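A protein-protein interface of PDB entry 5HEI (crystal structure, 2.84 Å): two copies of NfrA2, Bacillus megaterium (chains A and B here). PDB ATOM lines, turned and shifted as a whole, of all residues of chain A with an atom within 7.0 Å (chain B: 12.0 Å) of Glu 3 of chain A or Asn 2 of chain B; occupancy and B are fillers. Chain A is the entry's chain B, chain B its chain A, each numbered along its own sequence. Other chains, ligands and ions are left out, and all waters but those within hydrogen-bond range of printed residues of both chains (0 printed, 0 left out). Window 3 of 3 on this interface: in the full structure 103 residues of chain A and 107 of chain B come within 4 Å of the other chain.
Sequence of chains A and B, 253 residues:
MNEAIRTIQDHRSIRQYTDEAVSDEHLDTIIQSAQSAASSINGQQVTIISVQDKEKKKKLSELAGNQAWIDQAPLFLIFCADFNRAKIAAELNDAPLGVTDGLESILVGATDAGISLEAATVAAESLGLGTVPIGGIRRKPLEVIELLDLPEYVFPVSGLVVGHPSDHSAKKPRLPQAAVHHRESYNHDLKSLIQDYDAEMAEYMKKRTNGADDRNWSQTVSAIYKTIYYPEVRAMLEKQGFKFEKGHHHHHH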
ATOM      1  N   MET A   1      12.761   5.628   5.365  1.00  0.00           N
ATOM      2  CA  MET A   1      14.105   5.099   5.152  1.00  0.00           C
ATOM      3  C   MET A   1      14.587   5.428   3.732  1.00  0.00           C
ATOM      4  O   MET A   1      15.656   6.018   3.560  1.00  0.00           O
ATOM      5  CB  MET A   1      14.132   3.579   5.414  1.00  0.00           C
ATOM      6  CG  MET A   1      15.481   3.068   5.883  1.00  0.00           C
ATOM      7  SD  MET A   1      15.841   3.458   7.619  1.00  0.00           S
ATOM      8  CE  MET A   1      15.034   2.087   8.426  1.00  0.00           C
ATOM      9  N   ASN A   2      13.772   5.057   2.729  1.00  0.00           N
ATOM     10  CA  ASN A   2      13.990   5.262   1.296  1.00  0.00           C
ATOM     11  C   ASN A   2      12.979   6.261   0.697  1.00  0.00           C
ATOM     12  O   ASN A   2      11.978   6.592   1.343  1.00  0.00           O
ATOM     13  CB  ASN A   2      13.960   3.918   0.547  1.00  0.00           C
ATOM     14  CG  ASN A   2      12.723   3.080   0.790  1.00  0.00           C
ATOM     15  OD1 ASN A   2      11.607   3.439   0.406  1.00  0.00           O
ATOM     16  ND2 ASN A   2      12.907   1.920   1.398  1.00  0.00           N
ATOM     17  N   GLU A   3      13.251   6.729  -0.541  1.00  0.00           N
ATOM     18  CA  GLU A   3      12.448   7.707  -1.288  1.00  0.00           C
ATOM     19  C   GLU A   3      10.988   7.297  -1.487  1.00  0.00           C
ATOM     20  O   GLU A   3      10.110   8.160  -1.415  1.00  0.00           O
ATOM     21  CB  GLU A   3      13.122   8.059  -2.626  1.00  0.00           C
ATOM     22  CG  GLU A   3      12.628   9.346  -3.278  1.00  0.00           C
ATOM     23  CD  GLU A   3      13.550  10.002  -4.293  1.00  0.00           C
ATOM     24  OE1 GLU A   3      13.314  11.190  -4.615  1.00  0.00           O
ATOM     25  OE2 GLU A   3      14.505   9.341  -4.766  1.00  0.00           O
ATOM     26  N   ALA A   4      10.728   5.991  -1.706  1.00  0.00           N
ATOM     27  CA  ALA A   4       9.373   5.447  -1.873  1.00  0.00           C
ATOM     28  C   ALA A   4       8.567   5.581  -0.574  1.00  0.00           C
ATOM     29  O   ALA A   4       7.443   6.073  -0.618  1.00  0.00           O
ATOM     30  CB  ALA A   4       9.431   3.995  -2.315  1.00  0.00           C
ATOM     31  N   ILE A   5       9.161   5.195   0.579  1.00  0.00           N
ATOM     32  CA  ILE A   5       8.541   5.307   1.905  1.00  0.00           C
ATOM     33  C   ILE A   5       8.374   6.786   2.297  1.00  0.00           C
ATOM     34  O   ILE A   5       7.321   7.156   2.813  1.00  0.00           O
ATOM     35  CB  ILE A   5       9.267   4.426   2.972  1.00  0.00           C
ATOM     36  CG1 ILE A   5       9.061   2.928   2.658  1.00  0.00           C
ATOM     37  CG2 ILE A   5       8.808   4.749   4.410  1.00  0.00           C
ATOM     38  CD1 ILE A   5      10.046   1.988   3.304  1.00  0.00           C
ATOM     39  N   ARG A   6       9.378   7.634   1.991  1.00  0.00           N
ATOM     40  CA  ARG A   6       9.338   9.073   2.274  1.00  0.00           C
ATOM     41  C   ARG A   6       8.191   9.757   1.522  1.00  0.00           C
ATOM     42  O   ARG A   6       7.499  10.582   2.119  1.00  0.00           O
ATOM     43  CB  ARG A   6      10.678   9.745   1.944  1.00  0.00           C
ATOM     44  CG  ARG A   6      11.083  10.837   2.928  1.00  0.00           C
ATOM     45  CD  ARG A   6      12.307  10.425   3.729  1.00  0.00           C
ATOM     46  NE  ARG A   6      12.946  11.562   4.395  1.00  0.00           N
ATOM     47  CZ  ARG A   6      14.067  11.485   5.109  1.00  0.00           C
ATOM     48  NH1 ARG A   6      14.686  10.320   5.262  1.00  0.00           N
ATOM     49  NH2 ARG A   6      14.577  12.571   5.674  1.00  0.00           N
ATOM     50  N   THR A   7       7.960   9.381   0.236  1.00  0.00           N
ATOM     51  CA  THR A   7       6.883   9.931  -0.606  1.00  0.00           C
ATOM     52  C   THR A   7       5.518   9.637   0.029  1.00  0.00           C
ATOM     53  O   THR A   7       4.672  10.533   0.108  1.00  0.00           O
ATOM     54  CB  THR A   7       7.006   9.425  -2.060  1.00  0.00           C
ATOM     55  OG1 THR A   7       8.310   9.724  -2.555  1.00  0.00           O
ATOM     56  CG2 THR A   7       5.964  10.025  -2.995  1.00  0.00           C
ATOM     57  N   ILE A   8       5.322   8.391   0.504  1.00  0.00           N
ATOM     58  CA  ILE A   8       4.083   7.980   1.161  1.00  0.00           C
ATOM     59  C   ILE A   8       3.922   8.584   2.555  1.00  0.00           C
ATOM     60  O   ILE A   8       2.854   9.119   2.847  1.00  0.00           O
ATOM     61  CB  ILE A   8       3.736   6.456   1.049  1.00  0.00           C
ATOM     62  CG1 ILE A   8       2.417   6.105   1.752  1.00  0.00           C
ATOM     63  CG2 ILE A   8       4.845   5.527   1.490  1.00  0.00           C
ATOM     64  CD1 ILE A   8       1.139   6.712   1.127  1.00  0.00           C
ATOM     65  N   THR A  29       4.622   8.831 -17.295  1.00  0.00           N
ATOM     66  CA  THR A  29       5.261   8.223 -16.124  1.00  0.00           C
ATOM     67  C   THR A  29       4.205   7.810 -15.086  1.00  0.00           C
ATOM     68  O   THR A  29       4.312   6.724 -14.515  1.00  0.00           O
ATOM     69  CB  THR A  29       6.342   9.166 -15.563  1.00  0.00           C
ATOM     70  OG1 THR A  29       7.275   9.469 -16.602  1.00  0.00           O
ATOM     71  CG2 THR A  29       7.085   8.578 -14.365  1.00  0.00           C
ATOM     72  N   VAL A 122       1.641   7.952  -5.675  1.00  0.00           N
ATOM     73  CA  VAL A 122       3.076   7.917  -5.327  1.00  0.00           C
ATOM     74  C   VAL A 122       4.012   8.339  -6.458  1.00  0.00           C
ATOM     75  O   VAL A 122       5.075   8.895  -6.180  1.00  0.00           O
ATOM     76  CB  VAL A 122       3.585   6.647  -4.593  1.00  0.00           C
ATOM     77  CG1 VAL A 122       3.313   6.718  -3.096  1.00  0.00           C
ATOM     78  CG2 VAL A 122       3.025   5.368  -5.201  1.00  0.00           C
ATOM     79  N   ALA A 123       3.617   8.093  -7.725  1.00  0.00           N
ATOM     80  CA  ALA A 123       4.416   8.483  -8.889  1.00  0.00           C
ATOM     81  C   ALA A 123       4.359   9.998  -9.092  1.00  0.00           C
ATOM     82  O   ALA A 123       5.411  10.635  -9.185  1.00  0.00           O
ATOM     83  CB  ALA A 123       3.930   7.760 -10.138  1.00  0.00           C
ATOM     84  N   SER A 126       6.005  12.056  -6.151  1.00  0.00           N
ATOM     85  CA  SER A 126       7.472  11.950  -6.156  1.00  0.00           C
ATOM     86  C   SER A 126       8.098  12.856  -7.227  1.00  0.00           C
ATOM     87  O   SER A 126       9.259  13.253  -7.089  1.00  0.00           O
ATOM     88  CB  SER A 126       7.916  10.505  -6.344  1.00  0.00           C
ATOM     89  OG  SER A 126       7.527   9.998  -7.609  1.00  0.00           O
ATOM     90  N   LEU A 127       7.315  13.197  -8.276  1.00  0.00           N
ATOM     91  CA  LEU A 127       7.722  14.091  -9.366  1.00  0.00           C
ATOM     92  C   LEU A 127       7.616  15.575  -8.954  1.00  0.00           C
ATOM     93  O   LEU A 127       8.121  16.448  -9.661  1.00  0.00           O
ATOM     94  CB  LEU A 127       6.895  13.816 -10.639  1.00  0.00           C
ATOM     95  CG  LEU A 127       7.180  12.499 -11.374  1.00  0.00           C
ATOM     96  CD1 LEU A 127       6.005  12.088 -12.229  1.00  0.00           C
ATOM     97  CD2 LEU A 127       8.436  12.590 -12.220  1.00  0.00           C
ATOM     98  N   GLY A 128       6.984  15.829  -7.808  1.00  0.00           N
ATOM     99  CA  GLY A 128       6.798  17.168  -7.261  1.00  0.00           C
ATOM    100  C   GLY A 128       5.374  17.684  -7.331  1.00  0.00           C
ATOM    101  O   GLY A 128       5.060  18.714  -6.725  1.00  0.00           O
ATOM    102  N   MET B   1      14.552   7.951 -13.543  1.00  0.00           N
ATOM    103  CA  MET B   1      13.339   7.743 -12.749  1.00  0.00           C
ATOM    104  C   MET B   1      13.688   7.636 -11.259  1.00  0.00           C
ATOM    105  O   MET B   1      14.678   6.987 -10.909  1.00  0.00           O
ATOM    106  CB  MET B   1      12.561   6.490 -13.220  1.00  0.00           C
ATOM    107  CG  MET B   1      12.487   6.304 -14.746  1.00  0.00           C
ATOM    108  SD  MET B   1      11.850   7.722 -15.688  1.00  0.00           S
ATOM    109  CE  MET B   1      11.986   7.088 -17.347  1.00  0.00           C
ATOM    110  N   ASN B   2      12.879   8.278 -10.391  1.00  0.00           N
ATOM    111  CA  ASN B   2      13.052   8.319  -8.928  1.00  0.00           C
ATOM    112  C   ASN B   2      12.914   6.933  -8.278  1.00  0.00           C
ATOM    113  O   ASN B   2      12.283   6.058  -8.871  1.00  0.00           O
ATOM    114  CB  ASN B   2      12.032   9.281  -8.303  1.00  0.00           C
ATOM    115  CG  ASN B   2      12.022  10.663  -8.909  1.00  0.00           C
ATOM    116  OD1 ASN B   2      11.346  10.920  -9.911  1.00  0.00           O
ATOM    117  ND2 ASN B   2      12.756  11.589  -8.301  1.00  0.00           N
ATOM    118  N   GLU B   3      13.483   6.744  -7.050  1.00  0.00           N
ATOM    119  CA  GLU B   3      13.416   5.484  -6.284  1.00  0.00           C
ATOM    120  C   GLU B   3      11.963   5.043  -6.070  1.00  0.00           C
ATOM    121  O   GLU B   3      11.681   3.844  -6.104  1.00  0.00           O
ATOM    122  CB  GLU B   3      14.164   5.616  -4.945  1.00  0.00           C
ATOM    123  CG  GLU B   3      14.442   4.303  -4.223  1.00  0.00           C
ATOM    124  CD  GLU B   3      15.354   4.365  -3.007  1.00  0.00           C
ATOM    125  OE1 GLU B   3      15.630   3.285  -2.433  1.00  0.00           O
ATOM    126  OE2 GLU B   3      15.793   5.475  -2.624  1.00  0.00           O
ATOM    127  N   ALA B   4      11.046   6.012  -5.897  1.00  0.00           N
ATOM    128  CA  ALA B   4       9.615   5.753  -5.744  1.00  0.00           C
ATOM    129  C   ALA B   4       9.055   5.148  -7.036  1.00  0.00           C
ATOM    130  O   ALA B   4       8.428   4.092  -6.981  1.00  0.00           O
ATOM    131  CB  ALA B   4       8.883   7.039  -5.396  1.00  0.00           C
ATOM    132  N   ILE B   5       9.336   5.791  -8.195  1.00  0.00           N
ATOM    133  CA  ILE B   5       8.917   5.354  -9.534  1.00  0.00           C
ATOM    134  C   ILE B   5       9.559   3.999  -9.896  1.00  0.00           C
ATOM    135  O   ILE B   5       8.868   3.136 -10.430  1.00  0.00           O
ATOM    136  CB  ILE B   5       9.147   6.479 -10.593  1.00  0.00           C
ATOM    137  CG1 ILE B   5       8.181   7.662 -10.339  1.00  0.00           C
ATOM    138  CG2 ILE B   5       9.001   5.965 -12.041  1.00  0.00           C
ATOM    139  CD1 ILE B   5       8.623   8.991 -10.902  1.00  0.00           C
ATOM    140  N   ARG B   6      10.847   3.797  -9.555  1.00  0.00           N
ATOM    141  CA  ARG B   6      11.564   2.542  -9.809  1.00  0.00           C
ATOM    142  C   ARG B   6      11.070   1.383  -8.939  1.00  0.00           C
ATOM    143  O   ARG B   6      11.265   0.230  -9.319  1.00  0.00           O
ATOM    144  CB  ARG B   6      13.085   2.718  -9.714  1.00  0.00           C
ATOM    145  CG  ARG B   6      13.698   3.355 -10.959  1.00  0.00           C
ATOM    146  CD  ARG B   6      15.106   2.854 -11.231  1.00  0.00           C
ATOM    147  NE  ARG B   6      16.097   3.433 -10.320  1.00  0.00           N
ATOM    148  CZ  ARG B   6      17.380   3.086 -10.289  1.00  0.00           C
ATOM    149  NH1 ARG B   6      17.845   2.156 -11.117  1.00  0.00           N
ATOM    150  NH2 ARG B   6      18.208   3.663  -9.429  1.00  0.00           N
ATOM    151  N   THR B   7      10.406   1.680  -7.798  1.00  0.00           N
ATOM    152  CA  THR B   7       9.805   0.666  -6.917  1.00  0.00           C
ATOM    153  C   THR B   7       8.520   0.152  -7.572  1.00  0.00           C
ATOM    154  O   THR B   7       8.277  -1.059  -7.568  1.00  0.00           O
ATOM    155  CB  THR B   7       9.579   1.218  -5.492  1.00  0.00           C
ATOM    156  OG1 THR B   7      10.837   1.633  -4.952  1.00  0.00           O
ATOM    157  CG2 THR B   7       8.939   0.195  -4.549  1.00  0.00           C
ATOM    158  N   ILE B   8       7.718   1.071  -8.152  1.00  0.00           N
ATOM    159  CA  ILE B   8       6.458   0.743  -8.839  1.00  0.00           C
ATOM    160  C   ILE B   8       6.716   0.119 -10.225  1.00  0.00           C
ATOM    161  O   ILE B   8       6.129  -0.917 -10.519  1.00  0.00           O
ATOM    162  CB  ILE B   8       5.412   1.910  -8.907  1.00  0.00           C
ATOM    163  CG1 ILE B   8       5.387   2.803  -7.647  1.00  0.00           C
ATOM    164  CG2 ILE B   8       4.023   1.382  -9.226  1.00  0.00           C
ATOM    165  CD1 ILE B   8       5.153   4.283  -7.968  1.00  0.00           C
ATOM    166  N   GLN B   9       7.590   0.739 -11.054  1.00  0.00           N
ATOM    167  CA  GLN B   9       7.924   0.276 -12.410  1.00  0.00           C
ATOM    168  C   GLN B   9       8.503  -1.147 -12.465  1.00  0.00           C
ATOM    169  O   GLN B   9       8.176  -1.900 -13.385  1.00  0.00           O
ATOM    170  CB  GLN B   9       8.873   1.264 -13.111  1.00  0.00           C
ATOM    171  CG  GLN B   9       8.284   1.903 -14.365  1.00  0.00           C
ATOM    172  CD  GLN B   9       7.653   3.249 -14.112  1.00  0.00           C
ATOM    173  OE1 GLN B   9       6.834   3.426 -13.204  1.00  0.00           O
ATOM    174  NE2 GLN B   9       7.988   4.223 -14.945  1.00  0.00           N
ATOM    175  N   ASP B  10       9.357  -1.508 -11.482  1.00  0.00           N
ATOM    176  CA  ASP B  10      10.013  -2.816 -11.402  1.00  0.00           C
ATOM    177  C   ASP B  10       9.214  -3.850 -10.572  1.00  0.00           C
ATOM    178  O   ASP B  10       9.804  -4.798 -10.045  1.00  0.00           O
ATOM    179  CB  ASP B  10      11.460  -2.654 -10.883  1.00  0.00           C
ATOM    180  CG  ASP B  10      12.469  -3.581 -11.531  1.00  0.00           C
ATOM    181  OD1 ASP B  10      12.771  -3.386 -12.727  1.00  0.00           O
ATOM    182  OD2 ASP B  10      12.929  -4.523 -10.852  1.00  0.00           O
ATOM    183  N   HIS B  11       7.878  -3.684 -10.490  1.00  0.00           N
ATOM    184  CA  HIS B  11       7.015  -4.588  -9.734  1.00  0.00           C
ATOM    185  C   HIS B  11       6.913  -6.000 -10.304  1.00  0.00           C
ATOM    186  O   HIS B  11       6.664  -6.195 -11.497  1.00  0.00           O
ATOM    187  CB  HIS B  11       5.620  -3.990  -9.476  1.00  0.00           C
ATOM    188  CG  HIS B  11       4.674  -4.959  -8.827  1.00  0.00           C
ATOM    189  ND1 HIS B  11       4.785  -5.295  -7.485  1.00  0.00           N
ATOM    190  CD2 HIS B  11       3.669  -5.681  -9.373  1.00  0.00           C
ATOM    191  CE1 HIS B  11       3.837  -6.189  -7.259  1.00  0.00           C
ATOM    192  NE2 HIS B  11       3.138  -6.451  -8.364  1.00  0.00           N
ATOM    193  N   THR B  29       6.529  -0.102   9.665  1.00  0.00           N
ATOM    194  CA  THR B  29       6.770   0.766   8.508  1.00  0.00           C
ATOM    195  C   THR B  29       5.702   0.513   7.420  1.00  0.00           C
ATOM    196  O   THR B  29       5.215   1.472   6.822  1.00  0.00           O
ATOM    197  CB  THR B  29       8.218   0.601   8.019  1.00  0.00           C
ATOM    198  OG1 THR B  29       9.103   0.861   9.113  1.00  0.00           O
ATOM    199  CG2 THR B  29       8.561   1.521   6.849  1.00  0.00           C
ATOM    200  N   SER B  33       2.893   3.357   6.528  1.00  0.00           N
ATOM    201  CA  SER B  33       2.824   3.791   5.130  1.00  0.00           C
ATOM    202  C   SER B  33       1.395   3.620   4.598  1.00  0.00           C
ATOM    203  O   SER B  33       0.886   4.523   3.936  1.00  0.00           O
ATOM    204  CB  SER B  33       3.806   3.008   4.265  1.00  0.00           C
ATOM    205  OG  SER B  33       5.140   3.126   4.733  1.00  0.00           O
ATOM    206  N   SER B  36      -0.765   6.258   6.040  1.00  0.00           N
ATOM    207  CA  SER B  36      -0.369   7.532   5.435  1.00  0.00           C
ATOM    208  C   SER B  36      -1.084   7.846   4.115  1.00  0.00           C
ATOM    209  O   SER B  36      -1.129   9.007   3.713  1.00  0.00           O
ATOM    210  CB  SER B  36       1.145   7.586   5.254  1.00  0.00           C
ATOM    211  OG  SER B  36       1.804   7.639   6.508  1.00  0.00           O
ATOM    212  N   GLU B 118      -1.780  -1.177  -1.923  1.00  0.00           N
ATOM    213  CA  GLU B 118      -0.743  -0.653  -2.817  1.00  0.00           C
ATOM    214  C   GLU B 118       0.333   0.117  -2.046  1.00  0.00           C
ATOM    215  O   GLU B 118       1.514  -0.042  -2.353  1.00  0.00           O
ATOM    216  CB  GLU B 118      -1.365   0.196  -3.946  1.00  0.00           C
ATOM    217  CG  GLU B 118      -0.381   0.747  -4.976  1.00  0.00           C
ATOM    218  CD  GLU B 118       0.465  -0.232  -5.769  1.00  0.00           C
ATOM    219  OE1 GLU B 118       0.093  -1.426  -5.867  1.00  0.00           O
ATOM    220  OE2 GLU B 118       1.495   0.211  -6.325  1.00  0.00           O
ATOM    221  N   ALA B 119      -0.072   0.920  -1.034  1.00  0.00           N
ATOM    222  CA  ALA B 119       0.848   1.677  -0.177  1.00  0.00           C
ATOM    223  C   ALA B 119       1.686   0.693   0.636  1.00  0.00           C
ATOM    224  O   ALA B 119       2.899   0.872   0.748  1.00  0.00           O
ATOM    225  CB  ALA B 119       0.070   2.601   0.750  1.00  0.00           C
ATOM    226  N   THR B 121       2.310  -2.402  -0.309  1.00  0.00           N
ATOM    227  CA  THR B 121       3.117  -3.056  -1.347  1.00  0.00           C
ATOM    228  C   THR B 121       4.378  -2.230  -1.660  1.00  0.00           C
ATOM    229  O   THR B 121       5.481  -2.757  -1.519  1.00  0.00           O
ATOM    230  CB  THR B 121       2.245  -3.401  -2.578  1.00  0.00           C
ATOM    231  OG1 THR B 121       1.564  -4.628  -2.322  1.00  0.00           O
ATOM    232  CG2 THR B 121       3.044  -3.530  -3.880  1.00  0.00           C
ATOM    233  N   VAL B 122       4.220  -0.942  -2.053  1.00  0.00           N
ATOM    234  CA  VAL B 122       5.350  -0.060  -2.381  1.00  0.00           C
ATOM    235  C   VAL B 122       6.335   0.138  -1.220  1.00  0.00           C
ATOM    236  O   VAL B 122       7.533   0.253  -1.467  1.00  0.00           O
ATOM    237  CB  VAL B 122       4.984   1.264  -3.112  1.00  0.00           C
ATOM    238  CG1 VAL B 122       4.412   0.996  -4.499  1.00  0.00           C
ATOM    239  CG2 VAL B 122       4.036   2.128  -2.288  1.00  0.00           C
ATOM    240  N   ALA B 123       5.835   0.133   0.036  1.00  0.00           N
ATOM    241  CA  ALA B 123       6.656   0.260   1.243  1.00  0.00           C
ATOM    242  C   ALA B 123       7.444  -1.020   1.485  1.00  0.00           C
ATOM    243  O   ALA B 123       8.662  -0.952   1.653  1.00  0.00           O
ATOM    244  CB  ALA B 123       5.786   0.569   2.449  1.00  0.00           C
ATOM    245  N   ALA B 124       6.757  -2.184   1.474  1.00  0.00           N
ATOM    246  CA  ALA B 124       7.356  -3.505   1.682  1.00  0.00           C
ATOM    247  C   ALA B 124       8.397  -3.854   0.616  1.00  0.00           C
ATOM    248  O   ALA B 124       9.482  -4.313   0.970  1.00  0.00           O
ATOM    249  CB  ALA B 124       6.276  -4.570   1.732  1.00  0.00           C
ATOM    250  N   GLU B 125       8.080  -3.634  -0.677  1.00  0.00           N
ATOM    251  CA  GLU B 125       9.000  -3.929  -1.781  1.00  0.00           C
ATOM    252  C   GLU B 125      10.222  -2.997  -1.852  1.00  0.00           C
ATOM    253  O   GLU B 125      11.276  -3.424  -2.334  1.00  0.00           O
ATOM    254  CB  GLU B 125       8.271  -4.098  -3.127  1.00  0.00           C
ATOM    255  CG  GLU B 125       7.584  -5.450  -3.252  1.00  0.00           C
ATOM    256  CD  GLU B 125       6.907  -5.760  -4.574  1.00  0.00           C
ATOM    257  OE1 GLU B 125       5.953  -5.038  -4.942  1.00  0.00           O
ATOM    258  OE2 GLU B 125       7.289  -6.770  -5.211  1.00  0.00           O
ATOM    259  N   SER B 126      10.109  -1.756  -1.325  1.00  0.00           N
ATOM    260  CA  SER B 126      11.245  -0.831  -1.269  1.00  0.00           C
ATOM    261  C   SER B 126      12.220  -1.236  -0.153  1.00  0.00           C
ATOM    262  O   SER B 126      13.405  -0.906  -0.233  1.00  0.00           O
ATOM    263  CB  SER B 126      10.781   0.609  -1.084  1.00  0.00           C
ATOM    264  OG  SER B 126      10.145   0.792   0.170  1.00  0.00           O
ATOM    265  N   LEU B 127      11.719  -1.974   0.867  1.00  0.00           N
ATOM    266  CA  LEU B 127      12.511  -2.493   1.991  1.00  0.00           C
ATOM    267  C   LEU B 127      13.279  -3.772   1.599  1.00  0.00           C
ATOM    268  O   LEU B 127      14.148  -4.223   2.350  1.00  0.00           O
ATOM    269  CB  LEU B 127      11.619  -2.755   3.225  1.00  0.00           C
ATOM    270  CG  LEU B 127      11.067  -1.528   3.953  1.00  0.00           C
ATOM    271  CD1 LEU B 127       9.824  -1.881   4.745  1.00  0.00           C
ATOM    272  CD2 LEU B 127      12.108  -0.899   4.862  1.00  0.00           C
ATOM    273  N   GLY B 128      12.957  -4.322   0.426  1.00  0.00           N
ATOM    274  CA  GLY B 128      13.581  -5.523  -0.116  1.00  0.00           C
ATOM    275  C   GLY B 128      12.700  -6.753  -0.076  1.00  0.00           C
ATOM    276  O   GLY B 128      13.056  -7.783  -0.658  1.00  0.00           O
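OG of Ser 126 of chain B sits at hydrogen-bond distance from OD1 of Asn 2 of chain A (3.0 Å).
The backbone carbonyl oxygen of Glu 3 of chain B lies within hydrogen-bond range of the side-chain hydroxyl of Thr 7 of chain B, at 2.6 Å.
OG of Ser 33 of chain B is in hydrogen-bond range of O of Thr 29 of chain B (2.7 Å).
The backbone carbonyl oxygen (O) of Val 122 of chain B is in hydrogen-bond range of the side-chain hydroxyl (OG) of Ser 126 of chain B (3.1 Å).
OD1 of Asn 2 of chain A lies close to N of Ala 4 of chain A (3.4 Å).
OD1 of Asn 2 of chain A lies within hydrogen-bond range of N of Ile 5 of chain A, at 3.0 Å.
The side-chain hydroxyl (OG1) of Thr 7 of chain A is in hydrogen-bond range of the backbone carbonyl oxygen (O) of Glu 3 of chain A (2.6 Å).
Among the printed residues, merely in contact across the chains: Ile 8 of chain A with Ser 33 of chain B (3.1 Å), Ile 8 of chain A with Ser 36 of chain B (3.3 Å), Ile 5 of chain A with Ser 126 of chain B (3.4 Å), Asn 2 of chain A with Glu 3 of chain B (3.5 Å), Glu 3 of chain A with Glu 3 of chain B (3.5 Å), Ser 126 of chain A with Ile 5 of chain B (3.6 Å), Ile 5 of chain A with Ala 123 of chain B (3.6 Å), Val 122 of chain A with Ile 8 of chain B (3.7 Å), Ile 5 of chain A with Leu 127 of chain B (3.7 Å), Ser 126 of chain A with Ala 4 of chain B (3.7 Å), Glu 3 of chain A with Asn 2 of chain B (3.7 Å), Ala 4 of chain A with Thr 7 of chain B (3.8 Å), Thr 29 of chain A with Ile 5 of chain B (3.8 Å), Leu 127 of chain A with Ile 5 of chain B (3.8 Å), Ala 4 of chain A with Ser 126 of chain B (3.8 Å), Ala 4 of chain A with Ala 4 of chain B (3.9 Å), Ile 5 of chain A with Thr 29 of chain B (3.9 Å), Thr 7 of chain A with Ala 4 of chain B (3.95 Å) and Ala 123 of chain A with Ile 5 of chain B (3.996 Å).
Of chain A, only Glu 3 (3.7 Å) comes within 4 Å of Asn 2 of chain B.
Of the printed residues of chain B, Asn 2 of chain A touches Glu 3 (3.5 Å) and Ser 126 (3.0 Å).
Ala 4 of chain A touches three residues of chain B.
Ile 5 of chain A touches four residues of chain B.
Of chain B, only Ala 4 comes within 4 Å of Thr 7 of chain A.
Of the printed residues of chain B, Leu 127 of chain A touches Ile 5.
Of the printed residues of chain B, Thr 29 of chain A touches Ile 5.
Printed residues of chain A within 4 Å of Thr 29 of chain B: Ile 5 (3.9 Å).
Of the printed residues of chain A, Thr 7 of chain B touches Ala 4.
Of the printed residues of chain A, Ser 36 of chain B touches Ile 8.
His 11 of chain B touches none of the printed residues of chain A.
The nearest printed residue of chain B that does not touch Ile 8 of chain A is Ala 119 of chain B (4.3 Å).
Of the 14 printed residues of chain A, 11 touch a printed residue of chain B.
Hydrophobic or aromatic side chains of chain A within 4 Å of the printed part of chain B: Ala 4, Ile 5, Ile 8, Val 122 and Leu 127.
Along chain A the printed residues that touch a printed residue of chain B span positions 2 to 127.
Hydrophobic or aromatic side chains of chain B within 4 Å of the printed part of chain A: Ala 4, Ile 5, Ile 8 and Leu 127.
Asn 2 of chain A touches Glu 3 of chain B, and with the chains exchanged Glu 3 of chain A touches Asn 2 of chain B.
Glu 3 of chain B touches its own counterpart, Glu 3 of chain A.
Ala 4 of chain B touches its own counterpart, Ala 4 of chain A.
Val 122 of chain A touches Ile 8 of chain B, but with the chains exchanged Ile 8 of chain A does not touch Val 122 of chain B (5.1 Å).
Positions printed for both chains: 1, 2, 3, 4, 5, 6, 7, 8, 29, 122, 123, 126, 127 and 128.
Of the 20 pairs that touch across the chains among the printed residues, 16 have their exchanged pair printed and touching as well.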
